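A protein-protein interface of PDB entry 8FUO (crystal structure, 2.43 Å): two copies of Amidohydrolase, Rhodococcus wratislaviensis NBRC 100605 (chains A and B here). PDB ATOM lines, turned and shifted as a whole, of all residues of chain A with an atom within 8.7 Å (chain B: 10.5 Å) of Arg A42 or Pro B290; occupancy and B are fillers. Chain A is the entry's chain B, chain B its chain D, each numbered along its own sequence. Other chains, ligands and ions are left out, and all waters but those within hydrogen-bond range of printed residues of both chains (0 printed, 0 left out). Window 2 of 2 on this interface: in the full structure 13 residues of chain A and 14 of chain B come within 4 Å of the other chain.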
ATOM      1  N   LEU A  39     -23.821   5.152 -35.836  1.00  0.00           N
ATOM      2  CA  LEU A  39     -23.714   5.734 -34.503  1.00  0.00           C
ATOM      3  C   LEU A  39     -22.563   6.735 -34.440  1.00  0.00           C
ATOM      4  O   LEU A  39     -21.406   6.372 -34.692  1.00  0.00           O
ATOM      5  CB  LEU A  39     -23.523   4.639 -33.453  1.00  0.00           C
ATOM      6  CG  LEU A  39     -24.824   4.164 -32.825  1.00  0.00           C
ATOM      7  CD1 LEU A  39     -24.510   3.117 -31.794  1.00  0.00           C
ATOM      8  CD2 LEU A  39     -25.572   5.347 -32.227  1.00  0.00           C
ATOM      9  N   ASP A  40     -22.897   7.987 -34.106  1.00  0.00           N
ATOM     10  CA  ASP A  40     -21.905   8.956 -33.655  1.00  0.00           C
ATOM     11  C   ASP A  40     -21.036   8.328 -32.570  1.00  0.00           C
ATOM     12  O   ASP A  40     -21.525   7.566 -31.727  1.00  0.00           O
ATOM     13  CB  ASP A  40     -22.613  10.207 -33.117  1.00  0.00           C
ATOM     14  CG  ASP A  40     -21.646  11.317 -32.701  1.00  0.00           C
ATOM     15  OD1 ASP A  40     -22.102  12.476 -32.625  1.00  0.00           O
ATOM     16  OD2 ASP A  40     -20.449  11.062 -32.449  1.00  0.00           O
ATOM     17  N   ASP A  41     -19.742   8.671 -32.583  1.00  0.00           N
ATOM     18  CA  ASP A  41     -18.770   7.942 -31.772  1.00  0.00           C
ATOM     19  C   ASP A  41     -18.970   8.174 -30.272  1.00  0.00           C
ATOM     20  O   ASP A  41     -18.597   7.313 -29.457  1.00  0.00           O
ATOM     21  CB  ASP A  41     -17.347   8.325 -32.201  1.00  0.00           C
ATOM     22  CG  ASP A  41     -16.440   7.108 -32.414  1.00  0.00           C
ATOM     23  OD1 ASP A  41     -16.109   6.417 -31.418  1.00  0.00           O
ATOM     24  OD2 ASP A  41     -16.075   6.837 -33.589  1.00  0.00           O
ATOM     25  N   ARG A  42     -19.560   9.312 -29.881  1.00  0.00           N
ATOM     26  CA  ARG A  42     -19.805   9.551 -28.459  1.00  0.00           C
ATOM     27  C   ARG A  42     -20.761   8.521 -27.874  1.00  0.00           C
ATOM     28  O   ARG A  42     -20.672   8.198 -26.685  1.00  0.00           O
ATOM     29  CB  ARG A  42     -20.371  10.953 -28.232  1.00  0.00           C
ATOM     30  CG  ARG A  42     -21.890  11.021 -28.300  1.00  0.00           C
ATOM     31  CD  ARG A  42     -22.436  12.351 -27.781  1.00  0.00           C
ATOM     32  NE  ARG A  42     -22.709  12.322 -26.344  1.00  0.00           N
ATOM     33  CZ  ARG A  42     -23.300  13.316 -25.696  1.00  0.00           C
ATOM     34  NH1 ARG A  42     -23.507  13.230 -24.392  1.00  0.00           N
ATOM     35  NH2 ARG A  42     -23.666  14.409 -26.357  1.00  0.00           N
ATOM     36  N   TRP A  43     -21.671   7.990 -28.689  1.00  0.00           N
ATOM     37  CA  TRP A  43     -22.612   7.012 -28.173  1.00  0.00           C
ATOM     38  C   TRP A  43     -22.037   5.614 -28.170  1.00  0.00           C
ATOM     39  O   TRP A  43     -22.444   4.797 -27.337  1.00  0.00           O
ATOM     40  CB  TRP A  43     -23.897   7.044 -28.981  1.00  0.00           C
ATOM     41  CG  TRP A  43     -24.583   8.324 -28.806  1.00  0.00           C
ATOM     42  CD1 TRP A  43     -24.924   9.213 -29.782  1.00  0.00           C
ATOM     43  CD2 TRP A  43     -25.009   8.900 -27.563  1.00  0.00           C
ATOM     44  NE1 TRP A  43     -25.544  10.310 -29.225  1.00  0.00           N
ATOM     45  CE2 TRP A  43     -25.613  10.140 -27.863  1.00  0.00           C
ATOM     46  CE3 TRP A  43     -24.941   8.487 -26.223  1.00  0.00           C
ATOM     47  CZ2 TRP A  43     -26.152  10.970 -26.872  1.00  0.00           C
ATOM     48  CZ3 TRP A  43     -25.469   9.317 -25.240  1.00  0.00           C
ATOM     49  CH2 TRP A  43     -26.067  10.541 -25.572  1.00  0.00           C
ATOM     50  N   LYS A  44     -21.095   5.326 -29.076  1.00  0.00           N
ATOM     51  CA  LYS A  44     -20.464   4.010 -29.090  1.00  0.00           C
ATOM     52  C   LYS A  44     -19.668   3.782 -27.819  1.00  0.00           C
ATOM     53  O   LYS A  44     -19.653   2.663 -27.291  1.00  0.00           O
ATOM     54  CB  LYS A  44     -19.585   3.866 -30.337  1.00  0.00           C
ATOM     55  N   LYS A  45     -19.041   4.849 -27.300  1.00  0.00           N
ATOM     56  CA  LYS A  45     -18.292   4.828 -26.046  1.00  0.00           C
ATOM     57  C   LYS A  45     -19.217   4.756 -24.835  1.00  0.00           C
ATOM     58  O   LYS A  45     -18.953   3.994 -23.891  1.00  0.00           O
ATOM     59  CB  LYS A  45     -17.407   6.078 -25.958  1.00  0.00           C
ATOM     60  CG  LYS A  45     -16.774   6.319 -24.589  1.00  0.00           C
ATOM     61  CD  LYS A  45     -15.616   7.311 -24.643  1.00  0.00           C
ATOM     62  CE  LYS A  45     -16.114   8.740 -24.560  1.00  0.00           C
ATOM     63  NZ  LYS A  45     -14.988   9.706 -24.737  1.00  0.00           N
ATOM     64  N   HIS A  46     -20.290   5.563 -24.837  1.00  0.00           N
ATOM     65  CA  HIS A  46     -21.273   5.505 -23.759  1.00  0.00           C
ATOM     66  C   HIS A  46     -21.800   4.090 -23.589  1.00  0.00           C
ATOM     67  O   HIS A  46     -21.993   3.625 -22.459  1.00  0.00           O
ATOM     68  CB  HIS A  46     -22.421   6.486 -24.032  1.00  0.00           C
ATOM     69  CG  HIS A  46     -23.310   6.734 -22.853  1.00  0.00           C
ATOM     70  ND1 HIS A  46     -23.950   5.719 -22.171  1.00  0.00           N
ATOM     71  CD2 HIS A  46     -23.682   7.885 -22.244  1.00  0.00           C
ATOM     72  CE1 HIS A  46     -24.670   6.231 -21.190  1.00  0.00           C
ATOM     73  NE2 HIS A  46     -24.529   7.545 -21.216  1.00  0.00           N
ATOM     74  N   ILE A  47     -21.988   3.372 -24.703  1.00  0.00           N
ATOM     75  CA  ILE A  47     -22.456   1.989 -24.646  1.00  0.00           C
ATOM     76  C   ILE A  47     -21.389   1.061 -24.058  1.00  0.00           C
ATOM     77  O   ILE A  47     -21.712   0.108 -23.337  1.00  0.00           O
ATOM     78  CB  ILE A  47     -22.906   1.533 -26.040  1.00  0.00           C
ATOM     79  CG1 ILE A  47     -24.150   2.303 -26.455  1.00  0.00           C
ATOM     80  CG2 ILE A  47     -23.220   0.071 -26.042  1.00  0.00           C
ATOM     81  CD1 ILE A  47     -24.547   2.082 -27.899  1.00  0.00           C
ATOM     82  N   ARG A  48     -20.104   1.313 -24.347  1.00  0.00           N
ATOM     83  CA  ARG A  48     -19.052   0.460 -23.786  1.00  0.00           C
ATOM     84  C   ARG A  48     -18.960   0.624 -22.277  1.00  0.00           C
ATOM     85  O   ARG A  48     -18.680  -0.342 -21.556  1.00  0.00           O
ATOM     86  CB  ARG A  48     -17.690   0.767 -24.419  1.00  0.00           C
ATOM     87  CG  ARG A  48     -17.401   0.045 -25.731  1.00  0.00           C
ATOM     88  CD  ARG A  48     -15.904   0.085 -26.105  1.00  0.00           C
ATOM     89  NE  ARG A  48     -15.313   1.419 -25.986  1.00  0.00           N
ATOM     90  CZ  ARG A  48     -15.359   2.354 -26.934  1.00  0.00           C
ATOM     91  NH1 ARG A  48     -15.972   2.113 -28.084  1.00  0.00           N
ATOM     92  NH2 ARG A  48     -14.800   3.538 -26.725  1.00  0.00           N
ATOM     93  N   GLU A  49     -19.211   1.836 -21.783  1.00  0.00           N
ATOM     94  CA  GLU A  49     -19.030   2.124 -20.364  1.00  0.00           C
ATOM     95  C   GLU A  49     -20.265   1.736 -19.548  1.00  0.00           C
ATOM     96  O   GLU A  49     -20.166   0.988 -18.563  1.00  0.00           O
ATOM     97  CB  GLU A  49     -18.687   3.615 -20.181  1.00  0.00           C
ATOM     98  CG  GLU A  49     -17.307   4.015 -20.750  1.00  0.00           C
ATOM     99  CD  GLU A  49     -17.134   5.518 -20.988  1.00  0.00           C
ATOM    100  OE1 GLU A  49     -18.073   6.293 -20.716  1.00  0.00           O
ATOM    101  OE2 GLU A  49     -16.050   5.928 -21.454  1.00  0.00           O
ATOM    102  N   TYR A  50     -21.440   2.212 -19.963  1.00  0.00           N
ATOM    103  CA  TYR A  50     -22.653   2.069 -19.180  1.00  0.00           C
ATOM    104  C   TYR A  50     -23.654   1.069 -19.748  1.00  0.00           C
ATOM    105  O   TYR A  50     -24.574   0.667 -19.031  1.00  0.00           O
ATOM    106  CB  TYR A  50     -23.315   3.443 -19.031  1.00  0.00           C
ATOM    107  CG  TYR A  50     -22.487   4.401 -18.201  1.00  0.00           C
ATOM    108  CD1 TYR A  50     -22.646   4.456 -16.821  1.00  0.00           C
ATOM    109  CD2 TYR A  50     -21.547   5.244 -18.786  1.00  0.00           C
ATOM    110  CE1 TYR A  50     -21.905   5.321 -16.045  1.00  0.00           C
ATOM    111  CE2 TYR A  50     -20.795   6.119 -18.011  1.00  0.00           C
ATOM    112  CZ  TYR A  50     -20.982   6.148 -16.634  1.00  0.00           C
ATOM    113  OH  TYR A  50     -20.266   6.996 -15.825  1.00  0.00           O
ATOM    114  N   ASN A 123     -31.467   7.124 -20.661  1.00  0.00           N
ATOM    115  CA  ASN A 123     -30.744   8.170 -21.378  1.00  0.00           C
ATOM    116  C   ASN A 123     -31.459   8.432 -22.699  1.00  0.00           C
ATOM    117  O   ASN A 123     -31.221   7.748 -23.691  1.00  0.00           O
ATOM    118  CB  ASN A 123     -29.302   7.734 -21.610  1.00  0.00           C
ATOM    119  CG  ASN A 123     -28.416   8.873 -22.080  1.00  0.00           C
ATOM    120  OD1 ASN A 123     -28.859   9.815 -22.752  1.00  0.00           O
ATOM    121  ND2 ASN A 123     -27.149   8.800 -21.709  1.00  0.00           N
ATOM    122  N   GLU A 125     -31.215  10.758 -24.873  1.00  0.00           N
ATOM    123  CA  GLU A 125     -30.358  11.141 -25.992  1.00  0.00           C
ATOM    124  C   GLU A 125     -29.714   9.905 -26.593  1.00  0.00           C
ATOM    125  O   GLU A 125     -29.604   9.784 -27.815  1.00  0.00           O
ATOM    126  CB  GLU A 125     -29.284  12.144 -25.540  1.00  0.00           C
ATOM    127  CG  GLU A 125     -29.779  13.586 -25.241  1.00  0.00           C
ATOM    128  CD  GLU A 125     -30.731  13.692 -24.043  1.00  0.00           C
ATOM    129  OE1 GLU A 125     -31.702  14.479 -24.113  1.00  0.00           O
ATOM    130  OE2 GLU A 125     -30.524  12.982 -23.036  1.00  0.00           O
ATOM    131  N   LEU A 126     -29.300   8.971 -25.741  1.00  0.00           N
ATOM    132  CA  LEU A 126     -28.863   7.668 -26.224  1.00  0.00           C
ATOM    133  C   LEU A 126     -29.988   6.947 -26.967  1.00  0.00           C
ATOM    134  O   LEU A 126     -29.761   6.357 -28.033  1.00  0.00           O
ATOM    135  CB  LEU A 126     -28.364   6.826 -25.049  1.00  0.00           C
ATOM    136  CG  LEU A 126     -28.074   5.373 -25.417  1.00  0.00           C
ATOM    137  CD1 LEU A 126     -27.017   5.307 -26.531  1.00  0.00           C
ATOM    138  CD2 LEU A 126     -27.647   4.559 -24.197  1.00  0.00           C
ATOM    139  N   ALA A 129     -30.688   8.098 -30.398  1.00  0.00           N
ATOM    140  CA  ALA A 129     -29.552   7.749 -31.240  1.00  0.00           C
ATOM    141  C   ALA A 129     -29.685   6.327 -31.761  1.00  0.00           C
ATOM    142  O   ALA A 129     -29.622   6.089 -32.973  1.00  0.00           O
ATOM    143  CB  ALA A 129     -28.247   7.911 -30.458  1.00  0.00           C
ATOM    144  N   VAL B 248     -30.010  19.786 -12.051  1.00  0.00           N
ATOM    145  CA  VAL B 248     -28.607  20.164 -12.255  1.00  0.00           C
ATOM    146  C   VAL B 248     -27.950  19.258 -13.286  1.00  0.00           C
ATOM    147  O   VAL B 248     -27.491  19.721 -14.336  1.00  0.00           O
ATOM    148  CB  VAL B 248     -27.831  20.150 -10.916  1.00  0.00           C
ATOM    149  CG1 VAL B 248     -26.316  20.091 -11.154  1.00  0.00           C
ATOM    150  CG2 VAL B 248     -28.206  21.366 -10.024  1.00  0.00           C
ATOM    151  N   LEU B 249     -27.916  17.949 -13.005  1.00  0.00           N
ATOM    152  CA  LEU B 249     -27.171  16.990 -13.825  1.00  0.00           C
ATOM    153  C   LEU B 249     -27.781  16.811 -15.214  1.00  0.00           C
ATOM    154  O   LEU B 249     -27.118  16.261 -16.107  1.00  0.00           O
ATOM    155  CB  LEU B 249     -27.081  15.634 -13.107  1.00  0.00           C
ATOM    156  CG  LEU B 249     -26.290  15.488 -11.793  1.00  0.00           C
ATOM    157  CD1 LEU B 249     -26.733  14.245 -11.021  1.00  0.00           C
ATOM    158  CD2 LEU B 249     -24.763  15.441 -12.027  1.00  0.00           C
ATOM    159  N   SER B 250     -29.022  17.250 -15.415  1.00  0.00           N
ATOM    160  CA  SER B 250     -29.616  17.245 -16.751  1.00  0.00           C
ATOM    161  C   SER B 250     -29.112  18.374 -17.627  1.00  0.00           C
ATOM    162  O   SER B 250     -29.409  18.379 -18.825  1.00  0.00           O
ATOM    163  CB  SER B 250     -31.137  17.363 -16.682  1.00  0.00           C
ATOM    164  OG  SER B 250     -31.518  18.656 -16.240  1.00  0.00           O
ATOM    165  N   GLY B 251     -28.389  19.338 -17.062  1.00  0.00           N
ATOM    166  CA  GLY B 251     -28.062  20.531 -17.815  1.00  0.00           C
ATOM    167  C   GLY B 251     -29.268  21.364 -18.176  1.00  0.00           C
ATOM    168  O   GLY B 251     -29.244  22.067 -19.189  1.00  0.00           O
ATOM    169  N   ASP B 254     -27.911  24.845 -18.421  1.00  0.00           N
ATOM    170  CA  ASP B 254     -27.224  25.176 -19.666  1.00  0.00           C
ATOM    171  C   ASP B 254     -28.217  25.657 -20.722  1.00  0.00           C
ATOM    172  O   ASP B 254     -28.039  26.727 -21.314  1.00  0.00           O
ATOM    173  CB  ASP B 254     -26.416  23.973 -20.164  1.00  0.00           C
ATOM    174  CG  ASP B 254     -25.250  23.642 -19.237  1.00  0.00           C
ATOM    175  OD1 ASP B 254     -24.929  24.505 -18.402  1.00  0.00           O
ATOM    176  OD2 ASP B 254     -24.661  22.534 -19.326  1.00  0.00           O
ATOM    177  N   TRP B 282     -19.291  12.955  -9.055  1.00  0.00           N
ATOM    178  CA  TRP B 282     -19.092  13.480 -10.402  1.00  0.00           C
ATOM    179  C   TRP B 282     -17.617  13.533 -10.788  1.00  0.00           C
ATOM    180  O   TRP B 282     -17.287  13.452 -11.973  1.00  0.00           O
ATOM    181  CB  TRP B 282     -19.734  14.867 -10.499  1.00  0.00           C
ATOM    182  CG  TRP B 282     -19.380  15.648 -11.739  1.00  0.00           C
ATOM    183  CD1 TRP B 282     -20.095  15.716 -12.904  1.00  0.00           C
ATOM    184  CD2 TRP B 282     -18.232  16.479 -11.929  1.00  0.00           C
ATOM    185  NE1 TRP B 282     -19.463  16.537 -13.802  1.00  0.00           N
ATOM    186  CE2 TRP B 282     -18.313  17.015 -13.230  1.00  0.00           C
ATOM    187  CE3 TRP B 282     -17.136  16.820 -11.123  1.00  0.00           C
ATOM    188  CZ2 TRP B 282     -17.343  17.874 -13.743  1.00  0.00           C
ATOM    189  CZ3 TRP B 282     -16.172  17.666 -11.633  1.00  0.00           C
ATOM    190  CH2 TRP B 282     -16.288  18.196 -12.929  1.00  0.00           C
ATOM    191  N   LEU B 285     -17.177   9.970 -12.272  1.00  0.00           N
ATOM    192  CA  LEU B 285     -18.082   9.457 -13.300  1.00  0.00           C
ATOM    193  C   LEU B 285     -18.652  10.529 -14.223  1.00  0.00           C
ATOM    194  O   LEU B 285     -19.541  10.221 -15.028  1.00  0.00           O
ATOM    195  CB  LEU B 285     -19.221   8.678 -12.640  1.00  0.00           C
ATOM    196  CG  LEU B 285     -18.797   7.396 -11.930  1.00  0.00           C
ATOM    197  CD1 LEU B 285     -19.783   7.090 -10.848  1.00  0.00           C
ATOM    198  CD2 LEU B 285     -18.707   6.245 -12.919  1.00  0.00           C
ATOM    199  N   ARG B 286     -18.151  11.767 -14.146  1.00  0.00           N
ATOM    200  CA  ARG B 286     -18.496  12.887 -15.026  1.00  0.00           C
ATOM    201  C   ARG B 286     -18.681  12.533 -16.504  1.00  0.00           C
ATOM    202  O   ARG B 286     -19.457  13.186 -17.212  1.00  0.00           O
ATOM    203  CB  ARG B 286     -17.396  13.929 -14.916  1.00  0.00           C
ATOM    204  CG  ARG B 286     -16.021  13.259 -14.870  1.00  0.00           C
ATOM    205  CD  ARG B 286     -14.959  14.229 -14.421  1.00  0.00           C
ATOM    206  NE  ARG B 286     -15.077  15.461 -15.180  1.00  0.00           N
ATOM    207  CZ  ARG B 286     -14.348  16.547 -14.967  1.00  0.00           C
ATOM    208  NH1 ARG B 286     -14.544  17.618 -15.727  1.00  0.00           N
ATOM    209  NH2 ARG B 286     -13.438  16.563 -13.996  1.00  0.00           N
ATOM    210  N   GLY B 287     -17.951  11.523 -16.985  1.00  0.00           N
ATOM    211  CA  GLY B 287     -17.975  11.161 -18.390  1.00  0.00           C
ATOM    212  C   GLY B 287     -19.249  10.489 -18.863  1.00  0.00           C
ATOM    213  O   GLY B 287     -19.369  10.228 -20.063  1.00  0.00           O
ATOM    214  N   GLU B 288     -20.189  10.182 -17.963  1.00  0.00           N
ATOM    215  CA  GLU B 288     -21.495   9.725 -18.428  1.00  0.00           C
ATOM    216  C   GLU B 288     -22.281  10.868 -19.063  1.00  0.00           C
ATOM    217  O   GLU B 288     -23.058  10.642 -20.000  1.00  0.00           O
ATOM    218  CB  GLU B 288     -22.296   9.104 -17.277  1.00  0.00           C
ATOM    219  CG  GLU B 288     -23.555   8.343 -17.739  1.00  0.00           C
ATOM    220  CD  GLU B 288     -24.382   7.780 -16.592  1.00  0.00           C
ATOM    221  OE1 GLU B 288     -24.974   6.694 -16.764  1.00  0.00           O
ATOM    222  OE2 GLU B 288     -24.449   8.423 -15.517  1.00  0.00           O
ATOM    223  N   LEU B 289     -22.068  12.099 -18.587  1.00  0.00           N
ATOM    224  CA  LEU B 289     -22.831  13.273 -19.002  1.00  0.00           C
ATOM    225  C   LEU B 289     -21.883  14.348 -19.529  1.00  0.00           C
ATOM    226  O   LEU B 289     -21.776  15.436 -18.948  1.00  0.00           O
ATOM    227  CB  LEU B 289     -23.660  13.813 -17.837  1.00  0.00           C
ATOM    228  CG  LEU B 289     -24.592  12.840 -17.100  1.00  0.00           C
ATOM    229  CD1 LEU B 289     -25.443  13.566 -16.049  1.00  0.00           C
ATOM    230  CD2 LEU B 289     -25.474  12.076 -18.085  1.00  0.00           C
ATOM    231  N   PRO B 290     -21.207  14.091 -20.655  1.00  0.00           N
ATOM    232  CA  PRO B 290     -20.155  15.018 -21.104  1.00  0.00           C
ATOM    233  C   PRO B 290     -20.660  16.390 -21.525  1.00  0.00           C
ATOM    234  O   PRO B 290     -19.884  17.349 -21.481  1.00  0.00           O
ATOM    235  CB  PRO B 290     -19.516  14.276 -22.283  1.00  0.00           C
ATOM    236  CG  PRO B 290     -20.592  13.431 -22.804  1.00  0.00           C
ATOM    237  CD  PRO B 290     -21.428  13.005 -21.623  1.00  0.00           C
ATOM    238  N   ASP B 291     -21.917  16.536 -21.918  1.00  0.00           N
ATOM    239  CA  ASP B 291     -22.386  17.867 -22.288  1.00  0.00           C
ATOM    240  C   ASP B 291     -22.657  18.765 -21.088  1.00  0.00           C
ATOM    241  O   ASP B 291     -23.049  19.924 -21.279  1.00  0.00           O
ATOM    242  CB  ASP B 291     -23.649  17.773 -23.148  1.00  0.00           C
ATOM    243  CG  ASP B 291     -23.400  17.092 -24.482  1.00  0.00           C
ATOM    244  OD1 ASP B 291     -22.318  17.304 -25.077  1.00  0.00           O
ATOM    245  OD2 ASP B 291     -24.287  16.338 -24.929  1.00  0.00           O
ATOM    246  N   LEU B 292     -22.480  18.257 -19.865  1.00  0.00           N
ATOM    247  CA  LEU B 292     -22.621  19.088 -18.671  1.00  0.00           C
ATOM    248  C   LEU B 292     -21.493  20.111 -18.658  1.00  0.00           C
ATOM    249  O   LEU B 292     -20.310  19.753 -18.579  1.00  0.00           O
ATOM    250  CB  LEU B 292     -22.613  18.236 -17.404  1.00  0.00           C
ATOM    251  CG  LEU B 292     -23.060  19.003 -16.155  1.00  0.00           C
ATOM    252  CD1 LEU B 292     -24.361  19.767 -16.394  1.00  0.00           C
ATOM    253  CD2 LEU B 292     -23.197  18.061 -14.966  1.00  0.00           C
ATOM    254  N   GLN B 293     -21.862  21.386 -18.762  1.00  0.00           N
ATOM    255  CA  GLN B 293     -20.860  22.405 -19.027  1.00  0.00           C
ATOM    256  C   GLN B 293     -20.030  22.723 -17.794  1.00  0.00           C
ATOM    257  O   GLN B 293     -18.829  22.987 -17.917  1.00  0.00           O
ATOM    258  CB  GLN B 293     -21.537  23.650 -19.575  1.00  0.00           C
ATOM    259  CG  GLN B 293     -22.047  23.439 -20.988  1.00  0.00           C
ATOM    260  CD  GLN B 293     -22.994  24.536 -21.410  1.00  0.00           C
ATOM    261  OE1 GLN B 293     -22.978  25.634 -20.844  1.00  0.00           O
ATOM    262  NE2 GLN B 293     -23.840  24.247 -22.396  1.00  0.00           N
ATOM    263  N   ARG B 294     -20.627  22.661 -16.608  1.00  0.00           N
ATOM    264  CA  ARG B 294     -19.971  23.077 -15.381  1.00  0.00           C
ATOM    265  C   ARG B 294     -19.910  21.915 -14.396  1.00  0.00           C
ATOM    266  O   ARG B 294     -20.667  20.946 -14.495  1.00  0.00           O
ATOM    267  CB  ARG B 294     -20.705  24.271 -14.745  1.00  0.00           C
ATOM    268  CG  ARG B 294     -21.075  25.373 -15.743  1.00  0.00           C
ATOM    269  CD  ARG B 294     -22.089  26.396 -15.196  1.00  0.00           C
ATOM    270  NE  ARG B 294     -21.530  27.295 -14.185  1.00  0.00           N
ATOM    271  CZ  ARG B 294     -22.093  28.443 -13.807  1.00  0.00           C
ATOM    272  NH1 ARG B 294     -21.514  29.195 -12.877  1.00  0.00           N
ATOM    273  NH2 ARG B 294     -23.232  28.850 -14.360  1.00  0.00           N
ATOM    274  N   LYS B 295     -18.973  22.014 -13.461  1.00  0.00           N
ATOM    275  CA  LYS B 295     -19.006  21.164 -12.284  1.00  0.00           C
ATOM    276  C   LYS B 295     -20.365  21.322 -11.599  1.00  0.00           C
ATOM    277  O   LYS B 295     -20.901  22.436 -11.544  1.00  0.00           O
ATOM    278  CB  LYS B 295     -17.871  21.548 -11.330  1.00  0.00           C
ATOM    279  CG  LYS B 295     -17.444  20.458 -10.384  1.00  0.00           C
ATOM    280  CD  LYS B 295     -16.133  20.799  -9.693  1.00  0.00           C
ATOM    281  CE  LYS B 295     -16.272  22.050  -8.829  1.00  0.00           C
ATOM    282  NZ  LYS B 295     -15.519  21.938  -7.538  1.00  0.00           N
ATOM    283  N   TYR B 299     -23.733  25.423 -10.389  1.00  0.00           N
ATOM    284  CA  TYR B 299     -25.007  25.989 -10.793  1.00  0.00           C
ATOM    285  C   TYR B 299     -25.763  26.613  -9.624  1.00  0.00           C
ATOM    286  O   TYR B 299     -26.642  27.450  -9.859  1.00  0.00           O
ATOM    287  CB  TYR B 299     -25.862  24.917 -11.474  1.00  0.00           C
ATOM    288  CG  TYR B 299     -25.283  24.353 -12.760  1.00  0.00           C
ATOM    289  CD1 TYR B 299     -25.597  24.921 -13.988  1.00  0.00           C
ATOM    290  CD2 TYR B 299     -24.448  23.231 -12.745  1.00  0.00           C
ATOM    291  CE1 TYR B 299     -25.083  24.408 -15.171  1.00  0.00           C
ATOM    292  CE2 TYR B 299     -23.933  22.708 -13.917  1.00  0.00           C
ATOM    293  CZ  TYR B 299     -24.258  23.301 -15.126  1.00  0.00           C
ATOM    294  OH  TYR B 299     -23.759  22.805 -16.295  1.00  0.00           O
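The guanidinium group (NH2) of Arg A42 is in salt-bridge range of the side-chain carboxylate (OD2) of Asp B291, 2.5 Å away. OH of Tyr A50 lies close to O of Leu B285, 3.4 Å away.
The backbone NH (N) of Arg A42 sits close to the side-chain carboxylate (OD2) of Asp A40, at 3.2 Å. ND2 of Asn A123 lies within hydrogen-bond range of NE2 of His A46 (2.9 Å).
Among the printed residues, pairs that only touch across the chains: Arg A42 with Pro B290 (3.3 Å), His A46 with Glu B288 (3.6 Å) and Tyr A50 with Glu B288 (3.2 Å).
No residue of chain B comes within 4 Å of Asp A40. No residue of chain B comes within 4 Å of Asp A41. Arg A42 touches just these residues of chain B: Pro B290 and Asp B291. No residue of chain B comes within 4 Å of Lys A45. Of the printed residues of chain B, His A46 touches Glu B288. Of the printed residues of chain B, Tyr A50 touches Leu B285 (3.4 Å) and Glu B288 (3.2 Å). Trp B282 touches none of the printed residues of chain A. Printed residues of chain A within 4 Å of Leu B285: Tyr A50. Printed residues of chain A within 4 Å of Glu B288: His A46 (3.6 Å) and Tyr A50 (3.2 Å). Of chain A, only Arg A42 comes within 4 Å of Pro B290. Tyr B299 touches none of the printed residues of chain A. The nearest residue of chain A that does not touch Pro B290 is His A46 (5.6 Å). The nearest printed residue of chain A that does not touch Glu B288 is Asn A123 (4.8 Å).
Hydrophobic or aromatic side chains of chain B that line the printed part of chain A: Leu B285 and Pro B290. Along chain B the printed residues that touch a printed residue of chain A span positions 285 to 291. Of the 16 printed residues of chain A, 3 touch a printed residue of chain B. Hydrophobic or aromatic side chains of chain A within 4 Å of the printed part of chain B: His A46 and Tyr A50.
No position is printed for both chains.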
